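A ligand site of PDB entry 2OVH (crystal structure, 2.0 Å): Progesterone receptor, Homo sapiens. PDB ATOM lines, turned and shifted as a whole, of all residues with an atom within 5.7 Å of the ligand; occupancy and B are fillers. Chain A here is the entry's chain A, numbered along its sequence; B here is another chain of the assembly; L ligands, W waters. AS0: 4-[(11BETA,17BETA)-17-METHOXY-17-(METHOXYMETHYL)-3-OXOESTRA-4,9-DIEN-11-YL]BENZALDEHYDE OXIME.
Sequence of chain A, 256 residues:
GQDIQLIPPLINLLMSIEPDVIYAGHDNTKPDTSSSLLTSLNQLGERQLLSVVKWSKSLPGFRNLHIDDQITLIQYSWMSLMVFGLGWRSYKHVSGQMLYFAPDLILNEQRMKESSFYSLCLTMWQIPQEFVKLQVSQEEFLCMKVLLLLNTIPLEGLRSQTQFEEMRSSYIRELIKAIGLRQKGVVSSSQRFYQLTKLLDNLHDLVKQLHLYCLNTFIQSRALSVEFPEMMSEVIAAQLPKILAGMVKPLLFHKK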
ATOM      1  N   LEU A  38       7.857   7.815 -10.591  1.00  0.00           N
ATOM      2  CA  LEU A  38       8.387   9.060 -11.122  1.00  0.00           C
ATOM      3  C   LEU A  38       9.880   9.089 -10.833  1.00  0.00           C
ATOM      4  O   LEU A  38      10.683   9.531 -11.657  1.00  0.00           O
ATOM      5  CB  LEU A  38       7.697  10.272 -10.483  1.00  0.00           C
ATOM      6  CG  LEU A  38       6.188  10.398 -10.754  1.00  0.00           C
ATOM      7  CD1 LEU A  38       5.593  11.537  -9.918  1.00  0.00           C
ATOM      8  CD2 LEU A  38       5.944  10.645 -12.241  1.00  0.00           C
ATOM      9  N   LEU A  41      11.665   6.760 -13.280  1.00  0.00           N
ATOM     10  CA  LEU A  41      11.699   7.319 -14.632  1.00  0.00           C
ATOM     11  C   LEU A  41      12.788   8.382 -14.752  1.00  0.00           C
ATOM     12  O   LEU A  41      13.508   8.434 -15.757  1.00  0.00           O
ATOM     13  CB  LEU A  41      10.347   7.930 -15.007  1.00  0.00           C
ATOM     14  CG  LEU A  41       9.272   6.933 -15.440  1.00  0.00           C
ATOM     15  CD1 LEU A  41       7.950   7.665 -15.704  1.00  0.00           C
ATOM     16  CD2 LEU A  41       9.760   6.179 -16.683  1.00  0.00           C
ATOM     17  N   ASN A  42      12.916   9.228 -13.734  1.00  0.00           N
ATOM     18  CA  ASN A  42      13.929  10.274 -13.749  1.00  0.00           C
ATOM     19  C   ASN A  42      15.316   9.689 -13.676  1.00  0.00           C
ATOM     20  O   ASN A  42      16.256  10.178 -14.312  1.00  0.00           O
ATOM     21  CB  ASN A  42      13.741  11.270 -12.598  1.00  0.00           C
ATOM     22  CG  ASN A  42      12.522  12.144 -12.799  1.00  0.00           C
ATOM     23  OD1 ASN A  42      12.182  12.502 -13.924  1.00  0.00           O
ATOM     24  ND2 ASN A  42      11.861  12.495 -11.697  1.00  0.00           N
ATOM     25  N   GLN A  43      15.461   8.615 -12.911  1.00  0.00           N
ATOM     26  CA  GLN A  43      16.760   7.969 -12.825  1.00  0.00           C
ATOM     27  C   GLN A  43      17.083   7.312 -14.155  1.00  0.00           C
ATOM     28  O   GLN A  43      18.191   7.447 -14.659  1.00  0.00           O
ATOM     29  CB  GLN A  43      16.765   6.923 -11.697  1.00  0.00           C
ATOM     30  CG  GLN A  43      17.990   6.043 -11.702  1.00  0.00           C
ATOM     31  CD  GLN A  43      18.302   5.467 -10.337  1.00  0.00           C
ATOM     32  OE1 GLN A  43      18.998   6.087  -9.534  1.00  0.00           O
ATOM     33  NE2 GLN A  43      17.740   4.297 -10.049  1.00  0.00           N
ATOM     34  N   LEU A  44      16.107   6.595 -14.712  1.00  0.00           N
ATOM     35  CA  LEU A  44      16.297   5.926 -15.992  1.00  0.00           C
ATOM     36  C   LEU A  44      16.550   6.990 -17.049  1.00  0.00           C
ATOM     37  O   LEU A  44      17.387   6.810 -17.939  1.00  0.00           O
ATOM     38  CB  LEU A  44      15.060   5.125 -16.372  1.00  0.00           C
ATOM     39  CG  LEU A  44      15.089   4.390 -17.717  1.00  0.00           C
ATOM     40  CD1 LEU A  44      16.188   3.330 -17.708  1.00  0.00           C
ATOM     41  CD2 LEU A  44      13.718   3.772 -17.994  1.00  0.00           C
ATOM     42  N   GLY A  45      15.815   8.096 -16.947  1.00  0.00           N
ATOM     43  CA  GLY A  45      15.963   9.170 -17.913  1.00  0.00           C
ATOM     44  C   GLY A  45      17.365   9.761 -17.981  1.00  0.00           C
ATOM     45  O   GLY A  45      17.900   9.963 -19.078  1.00  0.00           O
ATOM     46  N   GLU A  46      17.954  10.048 -16.833  1.00  0.00           N
ATOM     47  CA  GLU A  46      19.293  10.620 -16.799  1.00  0.00           C
ATOM     48  C   GLU A  46      20.293   9.639 -17.397  1.00  0.00           C
ATOM     49  O   GLU A  46      21.199  10.038 -18.131  1.00  0.00           O
ATOM     50  CB  GLU A  46      19.711  10.982 -15.372  1.00  0.00           C
ATOM     51  CG  GLU A  46      20.978  11.831 -15.329  1.00  0.00           C
ATOM     52  CD  GLU A  46      21.247  12.456 -13.973  1.00  0.00           C
ATOM     53  OE1 GLU A  46      21.626  11.744 -13.035  1.00  0.00           O
ATOM     54  OE2 GLU A  46      21.060  13.688 -13.842  1.00  0.00           O
ATOM     55  N   GLN A  48      19.718   7.280 -19.626  1.00  0.00           N
ATOM     56  CA  GLN A  48      19.525   7.218 -21.067  1.00  0.00           C
ATOM     57  C   GLN A  48      20.112   8.451 -21.764  1.00  0.00           C
ATOM     58  O   GLN A  48      20.650   8.343 -22.867  1.00  0.00           O
ATOM     59  CB  GLN A  48      18.034   7.088 -21.389  1.00  0.00           C
ATOM     60  CG  GLN A  48      17.510   5.654 -21.222  1.00  0.00           C
ATOM     61  CD  GLN A  48      16.023   5.536 -21.516  1.00  0.00           C
ATOM     62  OE1 GLN A  48      15.421   6.415 -22.126  1.00  0.00           O
ATOM     63  NE2 GLN A  48      15.428   4.431 -21.079  1.00  0.00           N
ATOM     64  N   LEU A  49      20.009   9.618 -21.126  1.00  0.00           N
ATOM     65  CA  LEU A  49      20.545  10.853 -21.701  1.00  0.00           C
ATOM     66  C   LEU A  49      22.057  10.728 -21.904  1.00  0.00           C
ATOM     67  O   LEU A  49      22.580  11.018 -22.987  1.00  0.00           O
ATOM     68  CB  LEU A  49      20.231  12.048 -20.800  1.00  0.00           C
ATOM     69  CG  LEU A  49      20.761  13.412 -21.284  1.00  0.00           C
ATOM     70  CD1 LEU A  49      20.282  13.679 -22.707  1.00  0.00           C
ATOM     71  CD2 LEU A  49      20.289  14.508 -20.345  1.00  0.00           C
ATOM     72  N   TRP A  78      16.737  14.916 -27.483  1.00  0.00           N
ATOM     73  CA  TRP A  78      16.757  13.822 -26.502  1.00  0.00           C
ATOM     74  C   TRP A  78      15.392  13.235 -26.169  1.00  0.00           C
ATOM     75  O   TRP A  78      15.261  12.023 -26.031  1.00  0.00           O
ATOM     76  CB  TRP A  78      17.470  14.238 -25.200  1.00  0.00           C
ATOM     77  CG  TRP A  78      16.834  15.344 -24.390  1.00  0.00           C
ATOM     78  CD1 TRP A  78      17.181  16.666 -24.380  1.00  0.00           C
ATOM     79  CD2 TRP A  78      15.771  15.208 -23.430  1.00  0.00           C
ATOM     80  NE1 TRP A  78      16.390  17.347 -23.483  1.00  0.00           N
ATOM     81  CE2 TRP A  78      15.532  16.475 -22.885  1.00  0.00           C
ATOM     82  CE3 TRP A  78      14.998  14.122 -22.990  1.00  0.00           C
ATOM     83  CZ2 TRP A  78      14.565  16.699 -21.915  1.00  0.00           C
ATOM     84  CZ3 TRP A  78      14.032  14.338 -22.032  1.00  0.00           C
ATOM     85  CH2 TRP A  78      13.818  15.620 -21.493  1.00  0.00           C
ATOM     86  N   MET A  79      14.365  14.080 -26.030  1.00  0.00           N
ATOM     87  CA  MET A  79      13.028  13.571 -25.697  1.00  0.00           C
ATOM     88  C   MET A  79      12.494  12.666 -26.805  1.00  0.00           C
ATOM     89  O   MET A  79      11.991  11.582 -26.544  1.00  0.00           O
ATOM     90  CB  MET A  79      12.041  14.728 -25.469  1.00  0.00           C
ATOM     91  CG  MET A  79      10.642  14.285 -25.025  1.00  0.00           C
ATOM     92  SD  MET A  79      10.598  13.519 -23.387  1.00  0.00           S
ATOM     93  CE  MET A  79      10.537  14.968 -22.383  1.00  0.00           C
ATOM     94  N   MET A  82      14.420   9.387 -26.945  1.00  0.00           N
ATOM     95  CA  MET A  82      14.010   8.494 -25.869  1.00  0.00           C
ATOM     96  C   MET A  82      12.625   7.888 -26.060  1.00  0.00           C
ATOM     97  O   MET A  82      12.442   6.689 -25.834  1.00  0.00           O
ATOM     98  CB  MET A  82      14.053   9.231 -24.540  1.00  0.00           C
ATOM     99  CG  MET A  82      15.454   9.410 -24.022  1.00  0.00           C
ATOM    100  SD  MET A  82      15.471  10.269 -22.452  1.00  0.00           S
ATOM    101  CE  MET A  82      17.193  10.825 -22.453  1.00  0.00           C
ATOM    102  N   VAL A  83      11.636   8.679 -26.473  1.00  0.00           N
ATOM    103  CA  VAL A  83      10.315   8.118 -26.669  1.00  0.00           C
ATOM    104  C   VAL A  83      10.334   7.182 -27.889  1.00  0.00           C
ATOM    105  O   VAL A  83       9.583   6.207 -27.947  1.00  0.00           O
ATOM    106  CB  VAL A  83       9.231   9.211 -26.840  1.00  0.00           C
ATOM    107  CG1 VAL A  83       9.365   9.889 -28.192  1.00  0.00           C
ATOM    108  CG2 VAL A  83       7.847   8.600 -26.660  1.00  0.00           C
ATOM    109  N   LEU A  86      11.870   3.953 -26.696  1.00  0.00           N
ATOM    110  CA  LEU A  86      10.881   3.294 -25.850  1.00  0.00           C
ATOM    111  C   LEU A  86       9.907   2.547 -26.746  1.00  0.00           C
ATOM    112  O   LEU A  86       9.538   1.400 -26.471  1.00  0.00           O
ATOM    113  CB  LEU A  86      10.114   4.337 -25.042  1.00  0.00           C
ATOM    114  CG  LEU A  86       8.807   3.883 -24.383  1.00  0.00           C
ATOM    115  CD1 LEU A  86       9.083   2.798 -23.334  1.00  0.00           C
ATOM    116  CD2 LEU A  86       8.131   5.105 -23.759  1.00  0.00           C
ATOM    117  N   ARG A  89      11.613  -0.660 -28.190  1.00  0.00           N
ATOM    118  CA  ARG A  89      11.730  -1.735 -27.208  1.00  0.00           C
ATOM    119  C   ARG A  89      10.364  -2.375 -26.951  1.00  0.00           C
ATOM    120  O   ARG A  89      10.240  -3.606 -26.868  1.00  0.00           O
ATOM    121  CB  ARG A  89      12.328  -1.215 -25.893  1.00  0.00           C
ATOM    122  CG  ARG A  89      13.775  -0.733 -26.014  1.00  0.00           C
ATOM    123  CD  ARG A  89      14.387  -0.481 -24.636  1.00  0.00           C
ATOM    124  NE  ARG A  89      13.702   0.596 -23.927  1.00  0.00           N
ATOM    125  CZ  ARG A  89      13.962   1.890 -24.087  1.00  0.00           C
ATOM    126  NH1 ARG A  89      14.898   2.294 -24.943  1.00  0.00           N
ATOM    127  NH2 ARG A  89      13.271   2.775 -23.390  1.00  0.00           N
ATOM    128  N   TYR A 100       7.807  -0.691 -22.591  1.00  0.00           N
ATOM    129  CA  TYR A 100       9.049  -1.278 -22.127  1.00  0.00           C
ATOM    130  C   TYR A 100      10.098  -0.188 -21.931  1.00  0.00           C
ATOM    131  O   TYR A 100      10.984  -0.004 -22.768  1.00  0.00           O
ATOM    132  CB  TYR A 100       9.514  -2.312 -23.156  1.00  0.00           C
ATOM    133  CG  TYR A 100      10.591  -3.270 -22.697  1.00  0.00           C
ATOM    134  CD1 TYR A 100      11.894  -2.841 -22.478  1.00  0.00           C
ATOM    135  CD2 TYR A 100      10.314  -4.623 -22.541  1.00  0.00           C
ATOM    136  CE1 TYR A 100      12.896  -3.740 -22.126  1.00  0.00           C
ATOM    137  CE2 TYR A 100      11.305  -5.527 -22.196  1.00  0.00           C
ATOM    138  CZ  TYR A 100      12.587  -5.077 -21.987  1.00  0.00           C
ATOM    139  OH  TYR A 100      13.576  -5.984 -21.667  1.00  0.00           O
ATOM    140  N   PHE A 101      10.005   0.543 -20.821  1.00  0.00           N
ATOM    141  CA  PHE A 101      10.968   1.604 -20.538  1.00  0.00           C
ATOM    142  C   PHE A 101      12.355   0.987 -20.329  1.00  0.00           C
ATOM    143  O   PHE A 101      13.359   1.495 -20.810  1.00  0.00           O
ATOM    144  CB  PHE A 101      10.576   2.400 -19.293  1.00  0.00           C
ATOM    145  CG  PHE A 101       9.320   3.220 -19.452  1.00  0.00           C
ATOM    146  CD1 PHE A 101       8.086   2.707 -19.083  1.00  0.00           C
ATOM    147  CD2 PHE A 101       9.373   4.498 -19.966  1.00  0.00           C
ATOM    148  CE1 PHE A 101       6.934   3.461 -19.223  1.00  0.00           C
ATOM    149  CE2 PHE A 101       8.221   5.267 -20.116  1.00  0.00           C
ATOM    150  CZ  PHE A 101       7.003   4.746 -19.738  1.00  0.00           C
ATOM    151  N   PHE A 117       0.052   8.882 -14.281  1.00  0.00           N
ATOM    152  CA  PHE A 117       0.286   9.562 -15.539  1.00  0.00           C
ATOM    153  C   PHE A 117      -0.187   8.682 -16.691  1.00  0.00           C
ATOM    154  O   PHE A 117       0.539   8.445 -17.663  1.00  0.00           O
ATOM    155  CB  PHE A 117       1.778   9.927 -15.693  1.00  0.00           C
ATOM    156  CG  PHE A 117       2.726   8.799 -15.396  1.00  0.00           C
ATOM    157  CD1 PHE A 117       3.169   7.957 -16.407  1.00  0.00           C
ATOM    158  CD2 PHE A 117       3.224   8.614 -14.116  1.00  0.00           C
ATOM    159  CE1 PHE A 117       4.093   6.945 -16.135  1.00  0.00           C
ATOM    160  CE2 PHE A 117       4.142   7.615 -13.846  1.00  0.00           C
ATOM    161  CZ  PHE A 117       4.581   6.786 -14.858  1.00  0.00           C
ATOM    162  N   LEU A 120      -0.326  10.287 -20.267  1.00  0.00           N
ATOM    163  CA  LEU A 120       0.995  10.344 -20.875  1.00  0.00           C
ATOM    164  C   LEU A 120       1.320   8.975 -21.474  1.00  0.00           C
ATOM    165  O   LEU A 120       1.936   8.884 -22.541  1.00  0.00           O
ATOM    166  CB  LEU A 120       2.036  10.700 -19.829  1.00  0.00           C
ATOM    167  CG  LEU A 120       3.493  10.669 -20.310  1.00  0.00           C
ATOM    168  CD1 LEU A 120       3.789  11.849 -21.215  1.00  0.00           C
ATOM    169  CD2 LEU A 120       4.384  10.723 -19.114  1.00  0.00           C
ATOM    170  N   MET A 124       2.445   8.126 -25.409  1.00  0.00           N
ATOM    171  CA  MET A 124       3.687   7.448 -25.766  1.00  0.00           C
ATOM    172  C   MET A 124       3.426   6.100 -26.436  1.00  0.00           C
ATOM    173  O   MET A 124       4.185   5.647 -27.283  1.00  0.00           O
ATOM    174  CB  MET A 124       4.569   7.260 -24.531  1.00  0.00           C
ATOM    175  CG  MET A 124       4.944   8.570 -23.833  1.00  0.00           C
ATOM    176  SD  MET A 124       6.213   8.376 -22.560  1.00  0.00           S
ATOM    177  CE  MET A 124       5.302   7.580 -21.288  1.00  0.00           C
ATOM    178  N   LEU A 210       4.978  15.702 -24.478  1.00  0.00           N
ATOM    179  CA  LEU A 210       5.832  15.134 -23.448  1.00  0.00           C
ATOM    180  C   LEU A 210       6.553  16.210 -22.644  1.00  0.00           C
ATOM    181  O   LEU A 210       6.700  16.094 -21.433  1.00  0.00           O
ATOM    182  CB  LEU A 210       6.878  14.189 -24.074  1.00  0.00           C
ATOM    183  CG  LEU A 210       6.359  13.043 -24.954  1.00  0.00           C
ATOM    184  CD1 LEU A 210       7.532  12.172 -25.393  1.00  0.00           C
ATOM    185  CD2 LEU A 210       5.345  12.221 -24.197  1.00  0.00           C
ATOM    186  N   TYR A 213       4.135  17.735 -20.261  1.00  0.00           N
ATOM    187  CA  TYR A 213       3.900  16.869 -19.115  1.00  0.00           C
ATOM    188  C   TYR A 213       5.070  16.938 -18.151  1.00  0.00           C
ATOM    189  O   TYR A 213       4.877  16.919 -16.930  1.00  0.00           O
ATOM    190  CB  TYR A 213       3.664  15.427 -19.547  1.00  0.00           C
ATOM    191  CG  TYR A 213       2.899  14.660 -18.502  1.00  0.00           C
ATOM    192  CD1 TYR A 213       3.536  14.122 -17.386  1.00  0.00           C
ATOM    193  CD2 TYR A 213       1.514  14.533 -18.598  1.00  0.00           C
ATOM    194  CE1 TYR A 213       2.811  13.468 -16.398  1.00  0.00           C
ATOM    195  CE2 TYR A 213       0.782  13.884 -17.615  1.00  0.00           C
ATOM    196  CZ  TYR A 213       1.432  13.356 -16.513  1.00  0.00           C
ATOM    197  OH  TYR A 213       0.694  12.735 -15.541  1.00  0.00           O
ATOM    198  N   CYS A 214       6.281  17.014 -18.694  1.00  0.00           N
ATOM    199  CA  CYS A 214       7.481  17.102 -17.861  1.00  0.00           C
ATOM    200  C   CYS A 214       7.444  18.369 -17.013  1.00  0.00           C
ATOM    201  O   CYS A 214       7.709  18.334 -15.806  1.00  0.00           O
ATOM    202  CB  CYS A 214       8.726  17.122 -18.762  1.00  0.00           C
ATOM    203  SG  CYS A 214      10.289  17.030 -17.875  1.00  0.00           S
ATOM    204  N   LEU A 215       7.115  19.497 -17.636  1.00  0.00           N
ATOM    205  CA  LEU A 215       7.044  20.766 -16.934  1.00  0.00           C
ATOM    206  C   LEU A 215       5.991  20.748 -15.830  1.00  0.00           C
ATOM    207  O   LEU A 215       6.253  21.157 -14.697  1.00  0.00           O
ATOM    208  CB  LEU A 215       6.739  21.900 -17.926  1.00  0.00           C
ATOM    209  CG  LEU A 215       6.442  23.280 -17.322  1.00  0.00           C
ATOM    210  CD1 LEU A 215       7.602  23.722 -16.442  1.00  0.00           C
ATOM    211  CD2 LEU A 215       6.209  24.275 -18.447  1.00  0.00           C
ATOM    212  N   THR A 217       4.800  18.190 -14.329  1.00  0.00           N
ATOM    213  CA  THR A 217       5.179  17.247 -13.287  1.00  0.00           C
ATOM    214  C   THR A 217       6.123  17.989 -12.340  1.00  0.00           C
ATOM    215  O   THR A 217       6.067  17.822 -11.124  1.00  0.00           O
ATOM    216  CB  THR A 217       5.888  16.011 -13.870  1.00  0.00           C
ATOM    217  OG1 THR A 217       4.971  15.278 -14.696  1.00  0.00           O
ATOM    218  CG2 THR A 217       6.397  15.100 -12.761  1.00  0.00           C
ATOM    219  N   PHE A 218       6.975  18.832 -12.910  1.00  0.00           N
ATOM    220  CA  PHE A 218       7.914  19.614 -12.124  1.00  0.00           C
ATOM    221  C   PHE A 218       7.166  20.619 -11.250  1.00  0.00           C
ATOM    222  O   PHE A 218       7.376  20.692 -10.042  1.00  0.00           O
ATOM    223  CB  PHE A 218       8.870  20.382 -13.036  1.00  0.00           C
ATOM    224  CG  PHE A 218       9.819  21.262 -12.292  1.00  0.00           C
ATOM    225  CD1 PHE A 218      10.851  20.719 -11.551  1.00  0.00           C
ATOM    226  CD2 PHE A 218       9.659  22.639 -12.305  1.00  0.00           C
ATOM    227  CE1 PHE A 218      11.718  21.528 -10.839  1.00  0.00           C
ATOM    228  CE2 PHE A 218      10.513  23.465 -11.599  1.00  0.00           C
ATOM    229  CZ  PHE A 218      11.550  22.909 -10.856  1.00  0.00           C
ATOM    230  N   LEU B   5      19.918  20.563 -18.386  1.00  0.00           N
ATOM    231  CA  LEU B   5      20.490  19.423 -19.085  1.00  0.00           C
ATOM    232  C   LEU B   5      21.644  19.880 -19.971  1.00  0.00           C
ATOM    233  O   LEU B   5      22.559  19.107 -20.249  1.00  0.00           O
ATOM    234  CB  LEU B   5      19.429  18.712 -19.923  1.00  0.00           C
ATOM    235  CG  LEU B   5      18.243  18.139 -19.160  1.00  0.00           C
ATOM    236  CD1 LEU B   5      17.509  17.134 -20.035  1.00  0.00           C
ATOM    237  CD2 LEU B   5      18.722  17.463 -17.882  1.00  0.00           C
ATOM    238  N   ILE B   8      24.744  19.170 -18.360  1.00  0.00           N
ATOM    239  CA  ILE B   8      25.025  17.746 -18.340  1.00  0.00           C
ATOM    240  C   ILE B   8      25.461  17.276 -19.724  1.00  0.00           C
ATOM    241  O   ILE B   8      26.421  16.520 -19.858  1.00  0.00           O
ATOM    242  CB  ILE B   8      23.776  16.938 -17.927  1.00  0.00           C
ATOM    243  CG1 ILE B   8      23.346  17.331 -16.513  1.00  0.00           C
ATOM    244  CG2 ILE B   8      24.075  15.445 -17.985  1.00  0.00           C
ATOM    245  CD1 ILE B   8      22.074  16.643 -16.032  1.00  0.00           C
HETATM  246  C1  AS0 L   1       5.855  10.534 -16.121  1.00  0.00           C
HETATM  247  C3  AS0 L   1       7.378  12.233 -16.692  1.00  0.00           C
HETATM  248  C4  AS0 L   1       8.239  13.018 -17.762  1.00  0.00           C
HETATM  249  C5  AS0 L   1       7.379  13.386 -19.001  1.00  0.00           C
HETATM  250  C6  AS0 L   1       7.812  12.423 -20.181  1.00  0.00           C
HETATM  251  O2  AS0 L   1       6.666  11.109 -17.206  1.00  0.00           O
HETATM  252  C7  AS0 L   1       8.900  11.484 -19.655  1.00  0.00           C
HETATM  253  C8  AS0 L   1      10.091  10.883 -20.522  1.00  0.00           C
HETATM  254  C9  AS0 L   1       9.275  10.023 -21.523  1.00  0.00           C
HETATM  255  C10 AS0 L   1      10.233   9.239 -22.461  1.00  0.00           C
HETATM  256  C11 AS0 L   1      11.139   8.316 -21.668  1.00  0.00           C
HETATM  257  C12 AS0 L   1      11.529   7.142 -22.221  1.00  0.00           C
HETATM  258  C13 AS0 L   1      12.413   6.158 -21.494  1.00  0.00           C
HETATM  259  O14 AS0 L   1      12.761   5.106 -22.036  1.00  0.00           O
HETATM  260  C15 AS0 L   1      12.852   6.498 -20.056  1.00  0.00           C
HETATM  261  C16 AS0 L   1      12.414   7.870 -19.476  1.00  0.00           C
HETATM  262  C17 AS0 L   1      11.512   8.776 -20.292  1.00  0.00           C
HETATM  263  C18 AS0 L   1      11.071   9.956 -19.733  1.00  0.00           C
HETATM  264  C19 AS0 L   1      11.469  10.446 -18.304  1.00  0.00           C
HETATM  265  C20 AS0 L   1      10.331  11.237 -17.539  1.00  0.00           C
HETATM  266  C21 AS0 L   1       9.448  12.226 -18.428  1.00  0.00           C
HETATM  267  C22 AS0 L   1      10.440  13.340 -18.854  1.00  0.00           C
HETATM  268  C23 AS0 L   1      12.836  11.232 -18.279  1.00  0.00           C
HETATM  269  C24 AS0 L   1      13.590  11.478 -19.488  1.00  0.00           C
HETATM  270  C25 AS0 L   1      14.838  12.156 -19.439  1.00  0.00           C
HETATM  271  C26 AS0 L   1      15.363  12.609 -18.218  1.00  0.00           C
HETATM  272  C27 AS0 L   1      16.657  13.297 -18.222  1.00  0.00           C
HETATM  273  N28 AS0 L   1      17.204  13.745 -17.117  1.00  0.00           N
HETATM  274  O29 AS0 L   1      18.444  14.375 -17.194  1.00  0.00           O
HETATM  275  C30 AS0 L   1      14.638  12.390 -16.990  1.00  0.00           C
HETATM  276  C31 AS0 L   1      13.374  11.707 -17.037  1.00  0.00           C
HETATM  277  O32 AS0 L   1       8.828  14.193 -17.058  1.00  0.00           O
HETATM  278  C33 AS0 L   1       8.549  14.343 -15.603  1.00  0.00           C
HETATM  279  O   HOH W   1      16.257  12.996 -14.412  1.00  0.00           O
HETATM  280  O   HOH W   2      14.398   5.597 -24.275  1.00  0.00           O
HETATM  281  O   HOH W   3      19.305  14.980 -14.881  1.00  0.00           O
HETATM  282  O   HOH W   4      10.203  17.042 -14.117  1.00  0.00           O
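OG1 of Thr 217 lies within hydrogen-bond range of O of Tyr 213, at 2.8 Å. NH2 of Arg 89 is in hydrogen-bond range of O of Phe 101, at 2.9 Å. The side-chain amide nitrogen (ND2) of Asn 42 sits at hydrogen-bond distance from the backbone carbonyl oxygen (O) of Leu 38 (3.2 Å). The guanidinium group (NE) of Arg 89 lies within hydrogen-bond range of the backbone carbonyl oxygen (O) of Tyr 100 (3.0 Å).
NE2 of Gln 48 lies within hydrogen-bond range of O14 of the ligand, at 2.9 Å. NH2 of Arg 89 lies within hydrogen-bond range of O14 of the ligand. The side-chain sulfur (SG) of Cys 214 sits at hydrogen-bond distance from an oxygen (O32) of the ligand (3.3 Å).
Water W3 bridges OE2 of Glu 46 and O29 of the ligand. Water W1 bridges O of Asn 42 (2.8 Å) and N28 of the ligand (3.0 Å).
Merely in contact with the ligand: Leu 38, Leu 41, Asn 42, Leu 44, Gly 45, Glu 46, Leu 49, Trp 78, Met 79, Met 82, Phe 101, Phe 117, Leu 120, Met 124, Leu 210, Thr 217 and Leu 5 of chain B. Hydrophobic or aromatic side chains within 4 Å of the ligand: Leu 38, Leu 41, Leu 44, Leu 49, Trp 78, Met 79, Met 82, Phe 101, Phe 117, Leu 120, Met 124 and Leu 5 of chain B.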
